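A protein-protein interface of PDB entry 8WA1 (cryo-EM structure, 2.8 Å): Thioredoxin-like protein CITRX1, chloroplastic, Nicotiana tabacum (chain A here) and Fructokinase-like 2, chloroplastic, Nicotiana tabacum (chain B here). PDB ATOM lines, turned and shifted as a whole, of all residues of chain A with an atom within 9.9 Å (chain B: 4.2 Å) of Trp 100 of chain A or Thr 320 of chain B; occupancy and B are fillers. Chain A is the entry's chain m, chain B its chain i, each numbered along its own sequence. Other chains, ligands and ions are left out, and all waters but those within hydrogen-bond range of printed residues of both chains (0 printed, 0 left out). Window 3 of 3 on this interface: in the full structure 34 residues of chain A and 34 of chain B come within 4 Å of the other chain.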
ATOM      1  N   PHE A  96      11.499 -18.498  16.494  1.00  0.00           N
ATOM      2  CA  PHE A  96      12.101 -19.197  15.366  1.00  0.00           C
ATOM      3  C   PHE A  96      13.592 -19.359  15.635  1.00  0.00           C
ATOM      4  O   PHE A  96      14.307 -18.366  15.798  1.00  0.00           O
ATOM      5  CB  PHE A  96      11.864 -18.434  14.063  1.00  0.00           C
ATOM      6  CG  PHE A  96      10.430 -18.419  13.622  1.00  0.00           C
ATOM      7  CD1 PHE A  96       9.542 -17.490  14.136  1.00  0.00           C
ATOM      8  CD2 PHE A  96       9.970 -19.334  12.691  1.00  0.00           C
ATOM      9  CE1 PHE A  96       8.222 -17.476  13.731  1.00  0.00           C
ATOM     10  CE2 PHE A  96       8.651 -19.323  12.282  1.00  0.00           C
ATOM     11  CZ  PHE A  96       7.776 -18.393  12.802  1.00  0.00           C
ATOM     12  N   TYR A  97      14.042 -20.608  15.684  1.00  0.00           N
ATOM     13  CA  TYR A  97      15.427 -20.884  15.991  1.00  0.00           C
ATOM     14  C   TYR A  97      15.957 -21.930  15.071  1.00  0.00           C
ATOM     15  O   TYR A  97      15.195 -22.657  14.461  1.00  0.00           O
ATOM     16  CB  TYR A  97      15.547 -21.400  17.419  1.00  0.00           C
ATOM     17  CG  TYR A  97      15.230 -22.866  17.596  1.00  0.00           C
ATOM     18  CD1 TYR A  97      13.923 -23.314  17.626  1.00  0.00           C
ATOM     19  CD2 TYR A  97      16.244 -23.800  17.753  1.00  0.00           C
ATOM     20  CE1 TYR A  97      13.631 -24.651  17.785  1.00  0.00           C
ATOM     21  CE2 TYR A  97      15.960 -25.137  17.912  1.00  0.00           C
ATOM     22  CZ  TYR A  97      14.651 -25.554  17.931  1.00  0.00           C
ATOM     23  OH  TYR A  97      14.364 -26.885  18.095  1.00  0.00           O
ATOM     24  N   ALA A  98      17.268 -22.008  14.955  1.00  0.00           N
ATOM     25  CA  ALA A  98      17.872 -23.048  14.162  1.00  0.00           C
ATOM     26  C   ALA A  98      18.996 -23.559  15.002  1.00  0.00           C
ATOM     27  O   ALA A  98      19.601 -22.809  15.744  1.00  0.00           O
ATOM     28  CB  ALA A  98      18.403 -22.484  12.879  1.00  0.00           C
ATOM     29  N   THR A  99      19.296 -24.835  14.900  1.00  0.00           N
ATOM     30  CA  THR A  99      20.311 -25.390  15.758  1.00  0.00           C
ATOM     31  C   THR A  99      21.622 -24.727  15.467  1.00  0.00           C
ATOM     32  O   THR A  99      22.388 -24.434  16.372  1.00  0.00           O
ATOM     33  CB  THR A  99      20.462 -26.884  15.524  1.00  0.00           C
ATOM     34  OG1 THR A  99      20.945 -27.109  14.196  1.00  0.00           O
ATOM     35  CG2 THR A  99      19.123 -27.573  15.685  1.00  0.00           C
ATOM     36  N   TRP A 100      21.890 -24.474  14.199  1.00  0.00           N
ATOM     37  CA  TRP A 100      23.176 -23.934  13.844  1.00  0.00           C
ATOM     38  C   TRP A 100      23.494 -22.578  14.415  1.00  0.00           C
ATOM     39  O   TRP A 100      24.607 -22.362  14.860  1.00  0.00           O
ATOM     40  CB  TRP A 100      23.377 -23.962  12.328  1.00  0.00           C
ATOM     41  CG  TRP A 100      22.333 -23.313  11.536  1.00  0.00           C
ATOM     42  CD1 TRP A 100      21.226 -23.896  11.011  1.00  0.00           C
ATOM     43  CD2 TRP A 100      22.300 -21.947  11.135  1.00  0.00           C
ATOM     44  NE1 TRP A 100      20.491 -22.972  10.317  1.00  0.00           N
ATOM     45  CE2 TRP A 100      21.132 -21.764  10.382  1.00  0.00           C
ATOM     46  CE3 TRP A 100      23.145 -20.857  11.344  1.00  0.00           C
ATOM     47  CZ2 TRP A 100      20.785 -20.538   9.841  1.00  0.00           C
ATOM     48  CZ3 TRP A 100      22.797 -19.646  10.816  1.00  0.00           C
ATOM     49  CH2 TRP A 100      21.628 -19.491  10.075  1.00  0.00           C
ATOM     50  N   CYS A 101      22.543 -21.661  14.446  1.00  0.00           N
ATOM     51  CA  CYS A 101      22.882 -20.310  14.875  1.00  0.00           C
ATOM     52  C   CYS A 101      23.290 -20.187  16.313  1.00  0.00           C
ATOM     53  O   CYS A 101      22.675 -20.754  17.196  1.00  0.00           O
ATOM     54  CB  CYS A 101      21.775 -19.321  14.509  1.00  0.00           C
ATOM     55  SG  CYS A 101      20.927 -18.470  15.853  1.00  0.00           S
ATOM     56  N   GLY A 102      24.387 -19.499  16.550  1.00  0.00           N
ATOM     57  CA  GLY A 102      24.812 -19.254  17.905  1.00  0.00           C
ATOM     58  C   GLY A 102      23.941 -18.348  18.731  1.00  0.00           C
ATOM     59  O   GLY A 102      23.657 -18.639  19.885  1.00  0.00           O
ATOM     60  N   PRO A 103      23.491 -17.242  18.148  1.00  0.00           N
ATOM     61  CA  PRO A 103      22.723 -16.356  19.004  1.00  0.00           C
ATOM     62  C   PRO A 103      21.472 -17.018  19.524  1.00  0.00           C
ATOM     63  O   PRO A 103      21.075 -16.776  20.653  1.00  0.00           O
ATOM     64  CB  PRO A 103      22.372 -15.225  18.072  1.00  0.00           C
ATOM     65  CG  PRO A 103      23.542 -15.127  17.173  1.00  0.00           C
ATOM     66  CD  PRO A 103      23.953 -16.545  16.936  1.00  0.00           C
ATOM     67  N   CYS A 104      20.837 -17.834  18.712  1.00  0.00           N
ATOM     68  CA  CYS A 104      19.604 -18.437  19.135  1.00  0.00           C
ATOM     69  C   CYS A 104      19.791 -19.323  20.348  1.00  0.00           C
ATOM     70  O   CYS A 104      18.907 -19.410  21.185  1.00  0.00           O
ATOM     71  CB  CYS A 104      18.853 -19.109  17.993  1.00  0.00           C
ATOM     72  SG  CYS A 104      19.806 -19.925  16.711  1.00  0.00           S
ATOM     73  N   ILE A 105      20.932 -19.975  20.460  1.00  0.00           N
ATOM     74  CA  ILE A 105      21.194 -20.795  21.627  1.00  0.00           C
ATOM     75  C   ILE A 105      21.174 -19.956  22.892  1.00  0.00           C
ATOM     76  O   ILE A 105      20.666 -20.394  23.912  1.00  0.00           O
ATOM     77  CB  ILE A 105      22.513 -21.553  21.482  1.00  0.00           C
ATOM     78  CG1 ILE A 105      22.471 -22.407  20.219  1.00  0.00           C
ATOM     79  CG2 ILE A 105      22.787 -22.424  22.696  1.00  0.00           C
ATOM     80  CD1 ILE A 105      23.753 -23.156  19.945  1.00  0.00           C
ATOM     81  N   LEU A 106      21.701 -18.749  22.848  1.00  0.00           N
ATOM     82  CA  LEU A 106      21.613 -17.880  24.011  1.00  0.00           C
ATOM     83  C   LEU A 106      20.174 -17.481  24.281  1.00  0.00           C
ATOM     84  O   LEU A 106      19.708 -17.612  25.397  1.00  0.00           O
ATOM     85  CB  LEU A 106      22.428 -16.631  23.760  1.00  0.00           C
ATOM     86  CG  LEU A 106      23.945 -16.740  23.677  1.00  0.00           C
ATOM     87  CD1 LEU A 106      24.507 -15.790  22.636  1.00  0.00           C
ATOM     88  CD2 LEU A 106      24.556 -16.468  25.039  1.00  0.00           C
ATOM     89  N   ASP A 128      11.627 -24.960  14.824  1.00  0.00           N
ATOM     90  CA  ASP A 128      12.890 -25.049  14.102  1.00  0.00           C
ATOM     91  C   ASP A 128      12.724 -24.458  12.705  1.00  0.00           C
ATOM     92  O   ASP A 128      11.823 -24.853  11.958  1.00  0.00           O
ATOM     93  CB  ASP A 128      13.364 -26.500  14.033  1.00  0.00           C
ATOM     94  CG  ASP A 128      12.235 -27.473  13.755  1.00  0.00           C
ATOM     95  OD1 ASP A 128      11.100 -27.019  13.498  1.00  0.00           O
ATOM     96  OD2 ASP A 128      12.481 -28.696  13.802  1.00  0.00           O
ATOM     97  N   THR A 129      13.597 -23.510  12.357  1.00  0.00           N
ATOM     98  CA  THR A 129      13.468 -22.819  11.078  1.00  0.00           C
ATOM     99  C   THR A 129      13.892 -23.715   9.918  1.00  0.00           C
ATOM    100  O   THR A 129      13.313 -23.643   8.826  1.00  0.00           O
ATOM    101  CB  THR A 129      14.293 -21.530  11.102  1.00  0.00           C
ATOM    102  OG1 THR A 129      13.799 -20.669  12.136  1.00  0.00           O
ATOM    103  CG2 THR A 129      14.196 -20.804   9.775  1.00  0.00           C
ATOM    104  N   ASP A 130      14.893 -24.570  10.133  1.00  0.00           N
ATOM    105  CA  ASP A 130      15.385 -25.424   9.055  1.00  0.00           C
ATOM    106  C   ASP A 130      14.332 -26.442   8.630  1.00  0.00           C
ATOM    107  O   ASP A 130      14.176 -26.731   7.437  1.00  0.00           O
ATOM    108  CB  ASP A 130      16.675 -26.123   9.487  1.00  0.00           C
ATOM    109  CG  ASP A 130      16.534 -26.849  10.813  1.00  0.00           C
ATOM    110  OD1 ASP A 130      15.880 -27.913  10.847  1.00  0.00           O
ATOM    111  OD2 ASP A 130      17.079 -26.354  11.821  1.00  0.00           O
ATOM    112  N   ASP A 131      13.600 -27.004   9.594  1.00  0.00           N
ATOM    113  CA  ASP A 131      12.579 -27.992   9.262  1.00  0.00           C
ATOM    114  C   ASP A 131      11.350 -27.331   8.649  1.00  0.00           C
ATOM    115  O   ASP A 131      10.722 -27.893   7.745  1.00  0.00           O
ATOM    116  CB  ASP A 131      12.202 -28.791  10.510  1.00  0.00           C
ATOM    117  CG  ASP A 131      11.450 -30.073  10.187  1.00  0.00           C
ATOM    118  OD1 ASP A 131      10.386 -30.008   9.534  1.00  0.00           O
ATOM    119  OD2 ASP A 131      11.929 -31.153  10.589  1.00  0.00           O
ATOM    120  N   TYR A 133      10.697 -24.139   6.735  1.00  0.00           N
ATOM    121  CA  TYR A 133      11.240 -22.954   6.079  1.00  0.00           C
ATOM    122  C   TYR A 133      10.143 -22.137   5.407  1.00  0.00           C
ATOM    123  O   TYR A 133      10.185 -20.902   5.423  1.00  0.00           O
ATOM    124  CB  TYR A 133      12.320 -23.359   5.071  1.00  0.00           C
ATOM    125  CG  TYR A 133      11.942 -24.514   4.171  1.00  0.00           C
ATOM    126  CD1 TYR A 133      12.185 -25.828   4.552  1.00  0.00           C
ATOM    127  CD2 TYR A 133      11.354 -24.291   2.933  1.00  0.00           C
ATOM    128  CE1 TYR A 133      11.845 -26.886   3.732  1.00  0.00           C
ATOM    129  CE2 TYR A 133      11.010 -25.344   2.105  1.00  0.00           C
ATOM    130  CZ  TYR A 133      11.258 -26.638   2.509  1.00  0.00           C
ATOM    131  OH  TYR A 133      10.918 -27.688   1.689  1.00  0.00           O
ATOM    132  N   VAL A 141      10.099 -13.929   8.267  1.00  0.00           N
ATOM    133  CA  VAL A 141      11.257 -14.161   9.124  1.00  0.00           C
ATOM    134  C   VAL A 141      12.496 -13.731   8.348  1.00  0.00           C
ATOM    135  O   VAL A 141      12.945 -14.429   7.435  1.00  0.00           O
ATOM    136  CB  VAL A 141      11.351 -15.626   9.567  1.00  0.00           C
ATOM    137  CG1 VAL A 141      12.701 -15.903  10.217  1.00  0.00           C
ATOM    138  CG2 VAL A 141      10.227 -15.957  10.535  1.00  0.00           C
ATOM    139  N   ARG A 142      13.042 -12.568   8.705  1.00  0.00           N
ATOM    140  CA  ARG A 142      14.190 -12.041   7.975  1.00  0.00           C
ATOM    141  C   ARG A 142      15.502 -12.554   8.557  1.00  0.00           C
ATOM    142  O   ARG A 142      16.517 -12.610   7.854  1.00  0.00           O
ATOM    143  CB  ARG A 142      14.148 -10.514   7.980  1.00  0.00           C
ATOM    144  CG  ARG A 142      12.801  -9.958   7.553  1.00  0.00           C
ATOM    145  CD  ARG A 142      12.890  -8.492   7.177  1.00  0.00           C
ATOM    146  NE  ARG A 142      13.348  -7.664   8.288  1.00  0.00           N
ATOM    147  CZ  ARG A 142      13.532  -6.351   8.211  1.00  0.00           C
ATOM    148  NH1 ARG A 142      13.298  -5.712   7.073  1.00  0.00           N
ATOM    149  NH2 ARG A 142      13.950  -5.676   9.273  1.00  0.00           N
ATOM    150  N   GLY A 143      15.507 -12.950   9.818  1.00  0.00           N
ATOM    151  CA  GLY A 143      16.744 -13.375  10.435  1.00  0.00           C
ATOM    152  C   GLY A 143      16.567 -14.386  11.522  1.00  0.00           C
ATOM    153  O   GLY A 143      15.474 -14.585  12.012  1.00  0.00           O
ATOM    154  N   LEU A 144      17.633 -15.069  11.877  1.00  0.00           N
ATOM    155  CA  LEU A 144      17.491 -16.128  12.854  1.00  0.00           C
ATOM    156  C   LEU A 144      17.147 -15.806  14.296  1.00  0.00           C
ATOM    157  O   LEU A 144      16.322 -16.482  14.888  1.00  0.00           O
ATOM    158  CB  LEU A 144      18.631 -17.125  12.763  1.00  0.00           C
ATOM    159  CG  LEU A 144      18.277 -18.341  11.906  1.00  0.00           C
ATOM    160  CD1 LEU A 144      16.966 -18.929  12.396  1.00  0.00           C
ATOM    161  CD2 LEU A 144      18.161 -17.973  10.436  1.00  0.00           C
ATOM    162  N   PRO A 145      17.762 -14.782  14.882  1.00  0.00           N
ATOM    163  CA  PRO A 145      17.345 -14.569  16.270  1.00  0.00           C
ATOM    164  C   PRO A 145      16.123 -13.661  16.338  1.00  0.00           C
ATOM    165  O   PRO A 145      16.256 -12.537  16.793  1.00  0.00           O
ATOM    166  CB  PRO A 145      18.569 -13.937  16.913  1.00  0.00           C
ATOM    167  CG  PRO A 145      19.668 -14.067  15.907  1.00  0.00           C
ATOM    168  CD  PRO A 145      19.000 -14.059  14.580  1.00  0.00           C
ATOM    169  N   VAL B 291      21.738 -12.808  12.650  1.00  0.00           N
ATOM    170  CA  VAL B 291      22.200 -13.670  11.574  1.00  0.00           C
ATOM    171  C   VAL B 291      21.217 -13.552  10.417  1.00  0.00           C
ATOM    172  O   VAL B 291      20.038 -13.886  10.574  1.00  0.00           O
ATOM    173  CB  VAL B 291      22.332 -15.139  12.012  1.00  0.00           C
ATOM    174  CG1 VAL B 291      22.755 -16.007  10.838  1.00  0.00           C
ATOM    175  CG2 VAL B 291      23.319 -15.266  13.161  1.00  0.00           C
ATOM    176  N   SER B 293      21.101 -15.263   7.352  1.00  0.00           N
ATOM    177  CA  SER B 293      20.731 -16.584   6.861  1.00  0.00           C
ATOM    178  C   SER B 293      21.908 -17.527   7.075  1.00  0.00           C
ATOM    179  O   SER B 293      22.960 -17.135   7.588  1.00  0.00           O
ATOM    180  CB  SER B 293      20.317 -16.531   5.387  1.00  0.00           C
ATOM    181  OG  SER B 293      20.018 -17.828   4.898  1.00  0.00           O
ATOM    182  N   GLY B 294      21.721 -18.781   6.672  1.00  0.00           N
ATOM    183  CA  GLY B 294      22.752 -19.789   6.815  1.00  0.00           C
ATOM    184  C   GLY B 294      22.591 -20.941   5.844  1.00  0.00           C
ATOM    185  O   GLY B 294      21.474 -21.409   5.607  1.00  0.00           O
ATOM    186  N   ARG B 295      23.702 -21.405   5.272  1.00  0.00           N
ATOM    187  CA  ARG B 295      23.692 -22.480   4.293  1.00  0.00           C
ATOM    188  C   ARG B 295      24.739 -23.516   4.677  1.00  0.00           C
ATOM    189  O   ARG B 295      25.790 -23.159   5.232  1.00  0.00           O
ATOM    190  CB  ARG B 295      23.978 -21.960   2.878  1.00  0.00           C
ATOM    191  CG  ARG B 295      23.020 -20.880   2.406  1.00  0.00           C
ATOM    192  CD  ARG B 295      21.598 -21.405   2.302  1.00  0.00           C
ATOM    193  NE  ARG B 295      21.472 -22.460   1.300  1.00  0.00           N
ATOM    194  CZ  ARG B 295      20.333 -23.079   1.009  1.00  0.00           C
ATOM    195  NH1 ARG B 295      19.217 -22.750   1.645  1.00  0.00           N
ATOM    196  NH2 ARG B 295      20.308 -24.027   0.082  1.00  0.00           N
ATOM    197  N   PRO B 296      24.480 -24.795   4.411  1.00  0.00           N
ATOM    198  CA  PRO B 296      25.486 -25.825   4.690  1.00  0.00           C
ATOM    199  C   PRO B 296      26.778 -25.556   3.930  1.00  0.00           C
ATOM    200  O   PRO B 296      26.765 -25.175   2.758  1.00  0.00           O
ATOM    201  CB  PRO B 296      24.810 -27.117   4.216  1.00  0.00           C
ATOM    202  CG  PRO B 296      23.348 -26.820   4.271  1.00  0.00           C
ATOM    203  CD  PRO B 296      23.221 -25.371   3.911  1.00  0.00           C
ATOM    204  N   LYS B 318      26.448 -30.894  12.027  1.00  0.00           N
ATOM    205  CA  LYS B 318      26.293 -30.366  10.680  1.00  0.00           C
ATOM    206  C   LYS B 318      26.857 -28.954  10.640  1.00  0.00           C
ATOM    207  O   LYS B 318      26.375 -28.066  11.352  1.00  0.00           O
ATOM    208  CB  LYS B 318      24.822 -30.375  10.249  1.00  0.00           C
ATOM    209  CG  LYS B 318      23.852 -29.938  11.335  1.00  0.00           C
ATOM    210  CD  LYS B 318      22.410 -30.025  10.859  1.00  0.00           C
ATOM    211  CE  LYS B 318      21.441 -29.711  11.984  1.00  0.00           C
ATOM    212  NZ  LYS B 318      21.637 -30.618  13.148  1.00  0.00           N
ATOM    213  N   PHE B 319      27.879 -28.748   9.814  1.00  0.00           N
ATOM    214  CA  PHE B 319      28.568 -27.467   9.747  1.00  0.00           C
ATOM    215  C   PHE B 319      27.810 -26.515   8.832  1.00  0.00           C
ATOM    216  O   PHE B 319      27.634 -26.793   7.641  1.00  0.00           O
ATOM    217  CB  PHE B 319      30.003 -27.643   9.254  1.00  0.00           C
ATOM    218  CG  PHE B 319      30.802 -26.369   9.253  1.00  0.00           C
ATOM    219  CD1 PHE B 319      31.340 -25.873  10.428  1.00  0.00           C
ATOM    220  CD2 PHE B 319      31.013 -25.669   8.077  1.00  0.00           C
ATOM    221  CE1 PHE B 319      32.073 -24.702  10.430  1.00  0.00           C
ATOM    222  CE2 PHE B 319      31.746 -24.498   8.074  1.00  0.00           C
ATOM    223  CZ  PHE B 319      32.277 -24.014   9.252  1.00  0.00           C
ATOM    224  N   THR B 320      27.362 -25.396   9.397  1.00  0.00           N
ATOM    225  CA  THR B 320      26.647 -24.367   8.659  1.00  0.00           C
ATOM    226  C   THR B 320      27.164 -23.006   9.096  1.00  0.00           C
ATOM    227  O   THR B 320      27.236 -22.710  10.292  1.00  0.00           O
ATOM    228  CB  THR B 320      25.131 -24.456   8.893  1.00  0.00           C
ATOM    229  OG1 THR B 320      24.643 -25.715   8.418  1.00  0.00           O
ATOM    230  CG2 THR B 320      24.407 -23.330   8.172  1.00  0.00           C
ATOM    231  N   ARG B 321      27.520 -22.174   8.119  1.00  0.00           N
ATOM    232  CA  ARG B 321      28.081 -20.863   8.400  1.00  0.00           C
ATOM    233  C   ARG B 321      27.176 -19.783   7.826  1.00  0.00           C
ATOM    234  O   ARG B 321      26.340 -20.036   6.955  1.00  0.00           O
ATOM    235  CB  ARG B 321      29.497 -20.708   7.828  1.00  0.00           C
ATOM    236  CG  ARG B 321      29.543 -20.363   6.349  1.00  0.00           C
ATOM    237  CD  ARG B 321      30.940 -19.929   5.941  1.00  0.00           C
ATOM    238  NE  ARG B 321      31.925 -20.971   6.208  1.00  0.00           N
ATOM    239  CZ  ARG B 321      32.420 -21.787   5.284  1.00  0.00           C
ATOM    240  NH1 ARG B 321      32.030 -21.678   4.022  1.00  0.00           N
ATOM    241  NH2 ARG B 321      33.311 -22.708   5.621  1.00  0.00           N
ATOM    242  N   SER B 562      29.734 -21.186  16.660  1.00  0.00           N
ATOM    243  CA  SER B 562      29.585 -22.140  15.555  1.00  0.00           C
ATOM    244  C   SER B 562      29.106 -21.477  14.271  1.00  0.00           C
ATOM    245  O   SER B 562      29.391 -21.964  13.178  1.00  0.00           O
ATOM    246  CB  SER B 562      28.641 -23.276  15.943  1.00  0.00           C
ATOM    247  OG  SER B 562      27.336 -22.788  16.193  1.00  0.00           O
ATOM    248  N   ASP B 563      28.381 -20.375  14.392  1.00  0.00           N
ATOM    249  CA  ASP B 563      27.834 -19.682  13.225  1.00  0.00           C
ATOM    250  C   ASP B 563      28.867 -19.171  12.217  1.00  0.00           C
ATOM    251  O   ASP B 563      28.530 -19.033  11.044  1.00  0.00           O
ATOM    252  CB  ASP B 563      26.910 -18.540  13.669  1.00  0.00           C
ATOM    253  CG  ASP B 563      27.542 -17.637  14.724  1.00  0.00           C
ATOM    254  OD1 ASP B 563      28.765 -17.722  14.967  1.00  0.00           O
ATOM    255  OD2 ASP B 563      26.803 -16.822  15.312  1.00  0.00           O
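Trp 100 of chain A touches just these residues of chain B: Val 291 (3.6 Å), Ser 293 (3.6 Å), Gly 294 (3.5 Å), Thr 320 (3.9 Å) and Ser 562 (3.1 Å).
Thr 320 of chain B touches one residue of chain A.
Of chain A, only Trp 100 (3.6 Å) comes within 4 Å of Ser 293 of chain B.
Of chain A, only Trp 100 comes within 4 Å of Gly 294 of chain B.
Of the printed residues of chain A, Ser 562 of chain B touches Trp 100.
Of the printed residues of chain B, Thr 99 of chain A touches Lys 318 (3.5 Å).
Of the printed residues of chain B, Pro 103 of chain A touches Asp 563.
Of the printed residues of chain B, Pro 145 of chain A touches Val 291.
Printed residues of chain A within 4 Å of Val 291 of chain B: Trp 100 (3.6 Å), Gly 143 (3.3 Å), Leu 144 (3.0 Å) and Pro 145 (3.6 Å).
Of the printed residues of chain B, Gly 143 of chain A touches Val 291.
Ile 105 of chain A touches none of the printed residues of chain B.
Lys 318 of chain B touches Thr 99 of chain A (CE to OG1, 3.5 Å).
CZ3 of Trp 100 of chain A touches CG1 of Val 291 of chain B, at 3.6 Å.
CH2 of Trp 100 of chain A touches C of Ser 293 of chain B (3.6 Å).
CH2 of Trp 100 of chain A touches CA of Gly 294 of chain B (3.5 Å).
Trp 100 of chain A touches Thr 320 of chain B.
N of Gly 102 of chain A touches OD2 of Asp 563 of chain B (3.8 Å).
CD of Pro 103 of chain A touches OD2 of Asp 563 of chain B, 3.3 Å away.
Gly 143 of chain A touches Val 291 of chain B (CA to O, 3.3 Å).
CD of Pro 145 of chain A touches N of Val 291 of chain B (3.6 Å).
Of the 11 printed residues of chain B, 7 touch a printed residue of chain A.
Hydrophobic or aromatic side chains of chain A within 4 Å of the printed part of chain B: Trp 100, Pro 103 and Pro 145.
Among the printed residues, 11 pairs touch across the chains.
The backbone carbonyl oxygen of Trp 100 of chain A is in hydrogen-bond range of the side-chain hydroxyl of Ser 562 of chain B.
The backbone carbonyl oxygen of Val 291 of chain B lies within hydrogen-bond range of the backbone NH of Leu 144 of chain A.
The side-chain sulfur of Cys 101 of chain A forms a disulfide with the side-chain sulfur of Cys 104 of chain A, 2.0 Å away.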
